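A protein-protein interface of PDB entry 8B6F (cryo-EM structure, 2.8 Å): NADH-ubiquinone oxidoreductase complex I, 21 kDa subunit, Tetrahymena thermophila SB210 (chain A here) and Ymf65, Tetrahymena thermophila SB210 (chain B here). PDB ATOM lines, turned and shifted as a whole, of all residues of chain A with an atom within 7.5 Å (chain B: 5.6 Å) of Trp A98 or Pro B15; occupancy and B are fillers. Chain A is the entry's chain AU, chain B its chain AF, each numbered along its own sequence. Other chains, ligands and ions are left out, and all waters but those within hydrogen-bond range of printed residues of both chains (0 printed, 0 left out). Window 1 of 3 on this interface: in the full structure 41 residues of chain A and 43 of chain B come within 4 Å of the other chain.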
ATOM      1  N   LEU A  57      15.703   7.674   8.870  1.00  0.00           N
ATOM      2  CA  LEU A  57      16.213   8.116  10.164  1.00  0.00           C
ATOM      3  C   LEU A  57      16.715   6.933  10.983  1.00  0.00           C
ATOM      4  O   LEU A  57      17.769   7.015  11.622  1.00  0.00           O
ATOM      5  CB  LEU A  57      15.125   8.872  10.928  1.00  0.00           C
ATOM      6  CG  LEU A  57      14.883  10.326  10.511  1.00  0.00           C
ATOM      7  CD1 LEU A  57      13.624  10.866  11.163  1.00  0.00           C
ATOM      8  CD2 LEU A  57      16.078  11.198  10.865  1.00  0.00           C
ATOM      9  N   VAL A  58      15.968   5.829  10.982  1.00  0.00           N
ATOM     10  CA  VAL A  58      16.407   4.637  11.702  1.00  0.00           C
ATOM     11  C   VAL A  58      17.705   4.108  11.106  1.00  0.00           C
ATOM     12  O   VAL A  58      18.614   3.690  11.832  1.00  0.00           O
ATOM     13  CB  VAL A  58      15.297   3.570  11.689  1.00  0.00           C
ATOM     14  CG1 VAL A  58      15.789   2.265  12.295  1.00  0.00           C
ATOM     15  CG2 VAL A  58      14.076   4.071  12.437  1.00  0.00           C
ATOM     16  N   SER A  61      20.524   6.244  12.249  1.00  0.00           N
ATOM     17  CA  SER A  61      20.879   5.908  13.623  1.00  0.00           C
ATOM     18  C   SER A  61      21.692   4.623  13.681  1.00  0.00           C
ATOM     19  O   SER A  61      22.681   4.536  14.418  1.00  0.00           O
ATOM     20  CB  SER A  61      19.616   5.764  14.467  1.00  0.00           C
ATOM     21  OG  SER A  61      18.900   4.600  14.086  1.00  0.00           O
ATOM     22  N   TYR A  92      24.619  -0.120  21.075  1.00  0.00           N
ATOM     23  CA  TYR A  92      24.113  -0.069  19.708  1.00  0.00           C
ATOM     24  C   TYR A  92      22.593  -0.148  19.690  1.00  0.00           C
ATOM     25  O   TYR A  92      21.936   0.572  18.930  1.00  0.00           O
ATOM     26  CB  TYR A  92      24.731  -1.202  18.884  1.00  0.00           C
ATOM     27  CG  TYR A  92      24.707  -0.982  17.386  1.00  0.00           C
ATOM     28  CD1 TYR A  92      25.213   0.179  16.820  1.00  0.00           C
ATOM     29  CD2 TYR A  92      24.207  -1.957  16.537  1.00  0.00           C
ATOM     30  CE1 TYR A  92      25.199   0.372  15.451  1.00  0.00           C
ATOM     31  CE2 TYR A  92      24.188  -1.775  15.168  1.00  0.00           C
ATOM     32  CZ  TYR A  92      24.687  -0.608  14.632  1.00  0.00           C
ATOM     33  OH  TYR A  92      24.673  -0.422  13.271  1.00  0.00           O
ATOM     34  N   GLY A  93      22.017  -1.013  20.522  1.00  0.00           N
ATOM     35  CA  GLY A  93      20.568  -1.078  20.616  1.00  0.00           C
ATOM     36  C   GLY A  93      19.962   0.211  21.133  1.00  0.00           C
ATOM     37  O   GLY A  93      18.888   0.626  20.690  1.00  0.00           O
ATOM     38  N   GLY A  94      20.634   0.858  22.085  1.00  0.00           N
ATOM     39  CA  GLY A  94      20.159   2.144  22.566  1.00  0.00           C
ATOM     40  C   GLY A  94      20.153   3.210  21.488  1.00  0.00           C
ATOM     41  O   GLY A  94      19.207   3.993  21.383  1.00  0.00           O
ATOM     42  N   VAL A  95      21.211   3.262  20.675  1.00  0.00           N
ATOM     43  CA  VAL A  95      21.259   4.241  19.592  1.00  0.00           C
ATOM     44  C   VAL A  95      20.161   3.963  18.573  1.00  0.00           C
ATOM     45  O   VAL A  95      19.522   4.888  18.058  1.00  0.00           O
ATOM     46  CB  VAL A  95      22.652   4.251  18.938  1.00  0.00           C
ATOM     47  CG1 VAL A  95      22.670   5.185  17.738  1.00  0.00           C
ATOM     48  CG2 VAL A  95      23.711   4.662  19.946  1.00  0.00           C
ATOM     49  N   ILE A  96      19.928   2.689  18.256  1.00  0.00           N
ATOM     50  CA  ILE A  96      18.881   2.346  17.298  1.00  0.00           C
ATOM     51  C   ILE A  96      17.510   2.683  17.868  1.00  0.00           C
ATOM     52  O   ILE A  96      16.612   3.124  17.142  1.00  0.00           O
ATOM     53  CB  ILE A  96      18.987   0.863  16.898  1.00  0.00           C
ATOM     54  CG1 ILE A  96      20.301   0.615  16.152  1.00  0.00           C
ATOM     55  CG2 ILE A  96      17.802   0.452  16.029  1.00  0.00           C
ATOM     56  CD1 ILE A  96      20.609  -0.844  15.920  1.00  0.00           C
ATOM     57  N   LEU A  97      17.323   2.479  19.172  1.00  0.00           N
ATOM     58  CA  LEU A  97      16.063   2.859  19.802  1.00  0.00           C
ATOM     59  C   LEU A  97      15.867   4.367  19.752  1.00  0.00           C
ATOM     60  O   LEU A  97      14.751   4.851  19.531  1.00  0.00           O
ATOM     61  CB  LEU A  97      16.029   2.358  21.246  1.00  0.00           C
ATOM     62  CG  LEU A  97      14.665   1.923  21.791  1.00  0.00           C
ATOM     63  CD1 LEU A  97      14.803   1.441  23.223  1.00  0.00           C
ATOM     64  CD2 LEU A  97      13.640   3.043  21.699  1.00  0.00           C
ATOM     65  N   TRP A  98      16.946   5.128  19.938  1.00  0.00           N
ATOM     66  CA  TRP A  98      16.864   6.575  19.787  1.00  0.00           C
ATOM     67  C   TRP A  98      16.481   6.954  18.364  1.00  0.00           C
ATOM     68  O   TRP A  98      15.701   7.890  18.151  1.00  0.00           O
ATOM     69  CB  TRP A  98      18.194   7.217  20.175  1.00  0.00           C
ATOM     70  CG  TRP A  98      18.165   7.853  21.516  1.00  0.00           C
ATOM     71  CD1 TRP A  98      18.594   7.312  22.691  1.00  0.00           C
ATOM     72  CD2 TRP A  98      17.679   9.160  21.828  1.00  0.00           C
ATOM     73  NE1 TRP A  98      18.406   8.205  23.717  1.00  0.00           N
ATOM     74  CE2 TRP A  98      17.846   9.348  23.213  1.00  0.00           C
ATOM     75  CE3 TRP A  98      17.121  10.192  21.068  1.00  0.00           C
ATOM     76  CZ2 TRP A  98      17.473  10.525  23.855  1.00  0.00           C
ATOM     77  CZ3 TRP A  98      16.751  11.358  21.705  1.00  0.00           C
ATOM     78  CH2 TRP A  98      16.928  11.516  23.086  1.00  0.00           C
ATOM     79  N   GLY A  99      17.019   6.241  17.377  1.00  0.00           N
ATOM     80  CA  GLY A  99      16.603   6.469  16.005  1.00  0.00           C
ATOM     81  C   GLY A  99      15.125   6.201  15.801  1.00  0.00           C
ATOM     82  O   GLY A  99      14.442   6.944  15.093  1.00  0.00           O
ATOM     83  N   LEU A 100      14.614   5.131  16.410  1.00  0.00           N
ATOM     84  CA  LEU A 100      13.183   4.855  16.334  1.00  0.00           C
ATOM     85  C   LEU A 100      12.380   5.986  16.963  1.00  0.00           C
ATOM     86  O   LEU A 100      11.333   6.382  16.437  1.00  0.00           O
ATOM     87  CB  LEU A 100      12.866   3.528  17.024  1.00  0.00           C
ATOM     88  CG  LEU A 100      13.257   2.249  16.279  1.00  0.00           C
ATOM     89  CD1 LEU A 100      13.094   1.042  17.184  1.00  0.00           C
ATOM     90  CD2 LEU A 100      12.430   2.078  15.018  1.00  0.00           C
ATOM     91  N   VAL A 101      12.846   6.512  18.095  1.00  0.00           N
ATOM     92  CA  VAL A 101      12.150   7.620  18.742  1.00  0.00           C
ATOM     93  C   VAL A 101      12.146   8.845  17.839  1.00  0.00           C
ATOM     94  O   VAL A 101      11.132   9.542  17.717  1.00  0.00           O
ATOM     95  CB  VAL A 101      12.791   7.923  20.109  1.00  0.00           C
ATOM     96  CG1 VAL A 101      12.276   9.244  20.674  1.00  0.00           C
ATOM     97  CG2 VAL A 101      12.517   6.795  21.076  1.00  0.00           C
ATOM     98  N   LEU A 102      13.280   9.136  17.200  1.00  0.00           N
ATOM     99  CA  LEU A 102      13.337  10.273  16.287  1.00  0.00           C
ATOM    100  C   LEU A 102      12.398  10.075  15.105  1.00  0.00           C
ATOM    101  O   LEU A 102      11.753  11.026  14.649  1.00  0.00           O
ATOM    102  CB  LEU A 102      14.772  10.489  15.808  1.00  0.00           C
ATOM    103  CG  LEU A 102      15.768  10.971  16.868  1.00  0.00           C
ATOM    104  CD1 LEU A 102      17.171  11.031  16.294  1.00  0.00           C
ATOM    105  CD2 LEU A 102      15.369  12.325  17.432  1.00  0.00           C
ATOM    106  N   GLY A 103      12.318   8.852  14.583  1.00  0.00           N
ATOM    107  CA  GLY A 103      11.377   8.583  13.509  1.00  0.00           C
ATOM    108  C   GLY A 103       9.936   8.767  13.943  1.00  0.00           C
ATOM    109  O   GLY A 103       9.117   9.307  13.197  1.00  0.00           O
ATOM    110  N   PHE A 104       9.607   8.316  15.155  1.00  0.00           N
ATOM    111  CA  PHE A 104       8.264   8.527  15.683  1.00  0.00           C
ATOM    112  C   PHE A 104       7.954  10.014  15.802  1.00  0.00           C
ATOM    113  O   PHE A 104       6.859  10.460  15.442  1.00  0.00           O
ATOM    114  CB  PHE A 104       8.133   7.835  17.041  1.00  0.00           C
ATOM    115  CG  PHE A 104       6.779   7.979  17.678  1.00  0.00           C
ATOM    116  CD1 PHE A 104       6.480   9.080  18.465  1.00  0.00           C
ATOM    117  CD2 PHE A 104       5.814   7.000  17.513  1.00  0.00           C
ATOM    118  CE1 PHE A 104       5.242   9.209  19.059  1.00  0.00           C
ATOM    119  CE2 PHE A 104       4.574   7.125  18.104  1.00  0.00           C
ATOM    120  CZ  PHE A 104       4.288   8.230  18.879  1.00  0.00           C
ATOM    121  N   ASN A 105       8.912  10.798  16.302  1.00  0.00           N
ATOM    122  CA  ASN A 105       8.708  12.238  16.408  1.00  0.00           C
ATOM    123  C   ASN A 105       8.537  12.874  15.036  1.00  0.00           C
ATOM    124  O   ASN A 105       7.702  13.767  14.857  1.00  0.00           O
ATOM    125  CB  ASN A 105       9.879  12.876  17.152  1.00  0.00           C
ATOM    126  CG  ASN A 105       9.837  12.604  18.640  1.00  0.00           C
ATOM    127  OD1 ASN A 105       9.180  13.319  19.395  1.00  0.00           O
ATOM    128  ND2 ASN A 105      10.543  11.565  19.073  1.00  0.00           N
ATOM    129  N   ILE B  11       4.418  12.803  24.417  1.00  0.00           N
ATOM    130  CA  ILE B  11       5.479  12.770  23.414  1.00  0.00           C
ATOM    131  C   ILE B  11       6.835  13.048  24.055  1.00  0.00           C
ATOM    132  O   ILE B  11       7.832  12.389  23.738  1.00  0.00           O
ATOM    133  CB  ILE B  11       5.167  13.759  22.273  1.00  0.00           C
ATOM    134  CG1 ILE B  11       6.169  13.604  21.126  1.00  0.00           C
ATOM    135  CG2 ILE B  11       5.171  15.197  22.772  1.00  0.00           C
ATOM    136  CD1 ILE B  11       6.108  12.265  20.420  1.00  0.00           C
ATOM    137  N   PHE B  12       6.897  14.024  24.964  1.00  0.00           N
ATOM    138  CA  PHE B  12       8.177  14.421  25.538  1.00  0.00           C
ATOM    139  C   PHE B  12       8.749  13.368  26.478  1.00  0.00           C
ATOM    140  O   PHE B  12       9.942  13.419  26.789  1.00  0.00           O
ATOM    141  CB  PHE B  12       8.033  15.751  26.278  1.00  0.00           C
ATOM    142  CG  PHE B  12       9.345  16.407  26.607  1.00  0.00           C
ATOM    143  CD1 PHE B  12       9.995  16.132  27.798  1.00  0.00           C
ATOM    144  CD2 PHE B  12       9.929  17.299  25.722  1.00  0.00           C
ATOM    145  CE1 PHE B  12      11.203  16.733  28.101  1.00  0.00           C
ATOM    146  CE2 PHE B  12      11.136  17.902  26.018  1.00  0.00           C
ATOM    147  CZ  PHE B  12      11.773  17.619  27.208  1.00  0.00           C
ATOM    148  N   PHE B  13       7.932  12.425  26.947  1.00  0.00           N
ATOM    149  CA  PHE B  13       8.419  11.408  27.870  1.00  0.00           C
ATOM    150  C   PHE B  13       9.180  10.289  27.177  1.00  0.00           C
ATOM    151  O   PHE B  13       9.922   9.561  27.844  1.00  0.00           O
ATOM    152  CB  PHE B  13       7.251  10.807  28.658  1.00  0.00           C
ATOM    153  CG  PHE B  13       6.630  11.749  29.652  1.00  0.00           C
ATOM    154  CD1 PHE B  13       7.410  12.629  30.386  1.00  0.00           C
ATOM    155  CD2 PHE B  13       5.261  11.746  29.857  1.00  0.00           C
ATOM    156  CE1 PHE B  13       6.835  13.489  31.300  1.00  0.00           C
ATOM    157  CE2 PHE B  13       4.681  12.601  30.770  1.00  0.00           C
ATOM    158  CZ  PHE B  13       5.468  13.474  31.492  1.00  0.00           C
ATOM    159  N   LEU B  14       9.017  10.123  25.866  1.00  0.00           N
ATOM    160  CA  LEU B  14       9.671   9.006  25.188  1.00  0.00           C
ATOM    161  C   LEU B  14      11.188   9.094  25.253  1.00  0.00           C
ATOM    162  O   LEU B  14      11.829   8.087  25.600  1.00  0.00           O
ATOM    163  CB  LEU B  14       9.176   8.917  23.742  1.00  0.00           C
ATOM    164  CG  LEU B  14       7.665   8.756  23.562  1.00  0.00           C
ATOM    165  CD1 LEU B  14       7.320   8.668  22.088  1.00  0.00           C
ATOM    166  CD2 LEU B  14       7.139   7.537  24.306  1.00  0.00           C
ATOM    167  N   PRO B  15      11.828  10.225  24.937  1.00  0.00           N
ATOM    168  CA  PRO B  15      13.298  10.259  25.019  1.00  0.00           C
ATOM    169  C   PRO B  15      13.831   9.996  26.415  1.00  0.00           C
ATOM    170  O   PRO B  15      14.831   9.286  26.567  1.00  0.00           O
ATOM    171  CB  PRO B  15      13.643  11.676  24.534  1.00  0.00           C
ATOM    172  CG  PRO B  15      12.450  12.135  23.787  1.00  0.00           C
ATOM    173  CD  PRO B  15      11.281  11.504  24.457  1.00  0.00           C
ATOM    174  N   VAL B  16      13.197  10.560  27.444  1.00  0.00           N
ATOM    175  CA  VAL B  16      13.690  10.374  28.805  1.00  0.00           C
ATOM    176  C   VAL B  16      13.505   8.927  29.245  1.00  0.00           C
ATOM    177  O   VAL B  16      14.370   8.355  29.916  1.00  0.00           O
ATOM    178  CB  VAL B  16      13.005  11.357  29.772  1.00  0.00           C
ATOM    179  CG1 VAL B  16      13.341  12.788  29.391  1.00  0.00           C
ATOM    180  CG2 VAL B  16      11.500  11.153  29.789  1.00  0.00           C
ATOM    181  N   PHE B  17      12.376   8.313  28.882  1.00  0.00           N
ATOM    182  CA  PHE B  17      12.173   6.906  29.207  1.00  0.00           C
ATOM    183  C   PHE B  17      13.182   6.026  28.480  1.00  0.00           C
ATOM    184  O   PHE B  17      13.690   5.054  29.048  1.00  0.00           O
ATOM    185  CB  PHE B  17      10.744   6.483  28.862  1.00  0.00           C
ATOM    186  CG  PHE B  17       9.707   6.959  29.847  1.00  0.00           C
ATOM    187  CD1 PHE B  17      10.046   7.801  30.898  1.00  0.00           C
ATOM    188  CD2 PHE B  17       8.390   6.550  29.726  1.00  0.00           C
ATOM    189  CE1 PHE B  17       9.090   8.228  31.797  1.00  0.00           C
ATOM    190  CE2 PHE B  17       7.430   6.974  30.622  1.00  0.00           C
ATOM    191  CZ  PHE B  17       7.781   7.815  31.659  1.00  0.00           C
ATOM    192  N   THR B  18      13.483   6.346  27.221  1.00  0.00           N
ATOM    193  CA  THR B  18      14.488   5.581  26.492  1.00  0.00           C
ATOM    194  C   THR B  18      15.841   5.669  27.183  1.00  0.00           C
ATOM    195  O   THR B  18      16.519   4.656  27.380  1.00  0.00           O
ATOM    196  CB  THR B  18      14.581   6.086  25.053  1.00  0.00           C
ATOM    197  OG1 THR B  18      13.305   5.950  24.419  1.00  0.00           O
ATOM    198  CG2 THR B  18      15.618   5.299  24.263  1.00  0.00           C
ATOM    199  N   ASN B  19      16.249   6.879  27.567  1.00  0.00           N
ATOM    200  CA  ASN B  19      17.525   7.039  28.254  1.00  0.00           C
ATOM    201  C   ASN B  19      17.523   6.290  29.577  1.00  0.00           C
ATOM    202  O   ASN B  19      18.513   5.645  29.938  1.00  0.00           O
ATOM    203  CB  ASN B  19      17.825   8.518  28.479  1.00  0.00           C
ATOM    204  CG  ASN B  19      18.306   9.210  27.226  1.00  0.00           C
ATOM    205  OD1 ASN B  19      18.105   8.720  26.118  1.00  0.00           O
ATOM    206  ND2 ASN B  19      18.946  10.359  27.394  1.00  0.00           N
ATOM    207  N   LEU B  20      16.415   6.365  30.314  1.00  0.00           N
ATOM    208  CA  LEU B  20      16.323   5.667  31.589  1.00  0.00           C
ATOM    209  C   LEU B  20      16.457   4.163  31.394  1.00  0.00           C
ATOM    210  O   LEU B  20      17.200   3.494  32.120  1.00  0.00           O
ATOM    211  CB  LEU B  20      14.997   6.014  32.265  1.00  0.00           C
ATOM    212  CG  LEU B  20      14.820   5.578  33.718  1.00  0.00           C
ATOM    213  CD1 LEU B  20      15.798   6.299  34.629  1.00  0.00           C
ATOM    214  CD2 LEU B  20      13.392   5.831  34.163  1.00  0.00           C
ATOM    215  N   ILE B  22      17.912   2.522  28.893  1.00  0.00           N
ATOM    216  CA  ILE B  22      19.270   2.177  28.477  1.00  0.00           C
ATOM    217  C   ILE B  22      20.220   2.250  29.666  1.00  0.00           C
ATOM    218  O   ILE B  22      21.028   1.343  29.894  1.00  0.00           O
ATOM    219  CB  ILE B  22      19.724   3.094  27.328  1.00  0.00           C
ATOM    220  CG1 ILE B  22      18.833   2.887  26.102  1.00  0.00           C
ATOM    221  CG2 ILE B  22      21.176   2.816  26.959  1.00  0.00           C
ATOM    222  CD1 ILE B  22      18.952   3.982  25.068  1.00  0.00           C
ATOM    223  N   LEU B  66      24.234   9.865  25.557  1.00  0.00           N
ATOM    224  CA  LEU B  66      22.789  10.017  25.690  1.00  0.00           C
ATOM    225  C   LEU B  66      22.397  11.470  25.926  1.00  0.00           C
ATOM    226  O   LEU B  66      21.325  11.896  25.484  1.00  0.00           O
ATOM    227  CB  LEU B  66      22.246   9.110  26.796  1.00  0.00           C
ATOM    228  CG  LEU B  66      22.403   7.598  26.560  1.00  0.00           C
ATOM    229  CD1 LEU B  66      21.535   6.800  27.515  1.00  0.00           C
ATOM    230  CD2 LEU B  66      22.102   7.181  25.133  1.00  0.00           C
ATOM    231  N   LEU B  69      22.335  12.912  22.534  1.00  0.00           N
ATOM    232  CA  LEU B  69      21.118  12.510  21.840  1.00  0.00           C
ATOM    233  C   LEU B  69      19.923  13.320  22.327  1.00  0.00           C
ATOM    234  O   LEU B  69      19.049  13.687  21.534  1.00  0.00           O
ATOM    235  CB  LEU B  69      20.879  11.012  22.027  1.00  0.00           C
ATOM    236  CG  LEU B  69      21.924  10.105  21.370  1.00  0.00           C
ATOM    237  CD1 LEU B  69      21.685   8.653  21.732  1.00  0.00           C
ATOM    238  CD2 LEU B  69      21.926  10.273  19.859  1.00  0.00           C
ATOM    239  N   MET B  70      19.857  13.597  23.630  1.00  0.00           N
ATOM    240  CA  MET B  70      18.790  14.452  24.142  1.00  0.00           C
ATOM    241  C   MET B  70      18.914  15.864  23.585  1.00  0.00           C
ATOM    242  O   MET B  70      17.905  16.514  23.290  1.00  0.00           O
ATOM    243  CB  MET B  70      18.818  14.472  25.671  1.00  0.00           C
ATOM    244  CG  MET B  70      17.558  15.044  26.299  1.00  0.00           C
ATOM    245  SD  MET B  70      16.099  14.036  25.982  1.00  0.00           S
ATOM    246  CE  MET B  70      14.824  15.027  26.751  1.00  0.00           C
ATOM    247  N   TYR B  73      17.462  15.761  20.208  1.00  0.00           N
ATOM    248  CA  TYR B  73      16.006  15.781  20.288  1.00  0.00           C
ATOM    249  C   TYR B  73      15.492  17.193  20.529  1.00  0.00           C
ATOM    250  O   TYR B  73      14.515  17.622  19.903  1.00  0.00           O
ATOM    251  CB  TYR B  73      15.530  14.843  21.397  1.00  0.00           C
ATOM    252  CG  TYR B  73      14.057  14.965  21.700  1.00  0.00           C
ATOM    253  CD1 TYR B  73      13.114  14.328  20.909  1.00  0.00           C
ATOM    254  CD2 TYR B  73      13.612  15.708  22.783  1.00  0.00           C
ATOM    255  CE1 TYR B  73      11.766  14.437  21.183  1.00  0.00           C
ATOM    256  CE2 TYR B  73      12.267  15.824  23.066  1.00  0.00           C
ATOM    257  CZ  TYR B  73      11.350  15.184  22.263  1.00  0.00           C
ATOM    258  OH  TYR B  73      10.009  15.294  22.539  1.00  0.00           O
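The indole nitrogen (NE1) of Trp A98 is in hydrogen-bond range of the side-chain amide oxygen (OD1) of Asn B19, at 2.5 Å.
ND2 of Asn A105 is in hydrogen-bond range of O of Val A101, 2.5 Å away. The side-chain amide oxygen of Asn B19 lies close to the backbone carbonyl oxygen of Pro B15 (3.4 Å). The side-chain amide nitrogen (ND2) of Asn B19 sits at hydrogen-bond distance from the backbone carbonyl oxygen (O) of Leu B66 (3.4 Å). The backbone carbonyl oxygen of Leu B14 sits at hydrogen-bond distance from the side-chain hydroxyl of Thr B18 (2.9 Å).
Among the printed residues, pairs that only touch across the chains: Gly A94 with Ile B22, Leu A97 with Thr B18, Trp A98 with Pro B15, Trp A98 with Thr B18, Trp A98 with Leu B69, Trp A98 with Met B70, Trp A98 with Tyr B73, Val A101 with Thr B18, Phe A104 with Ile B11, Phe A104 with Leu B14, Asn A105 with Ile B11 and Asn A105 with Tyr B73.
Leu A57 touches none of the printed residues of chain B. Trp A98 touches just these residues of chain B: Pro B15 (3.6 Å), Thr B18 (3.9 Å), Asn B19 (2.5 Å), Leu B69 (3.3 Å), Met B70 (3.6 Å) and Tyr B73 (3.7 Å). Of the printed residues of chain B, Phe A104 touches Ile B11 (3.5 Å) and Leu B14 (3.7 Å). Pro B15 touches one residue of chain A. Of the printed residues of chain A, Thr B18 touches Leu A97, Trp A98 and Val A101. Of the printed residues of chain A, Met B70 touches Trp A98. The nearest residue of chain A that does not touch Pro B15 is Val A101 (4.3 Å). The nearest printed residue of chain A that does not touch Ile B22 is Trp A98 (4.1 Å).
Along chain A the printed residues that touch a printed residue of chain B span positions 94 to 105. Among the printed residues, 13 pairs touch across the chains.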
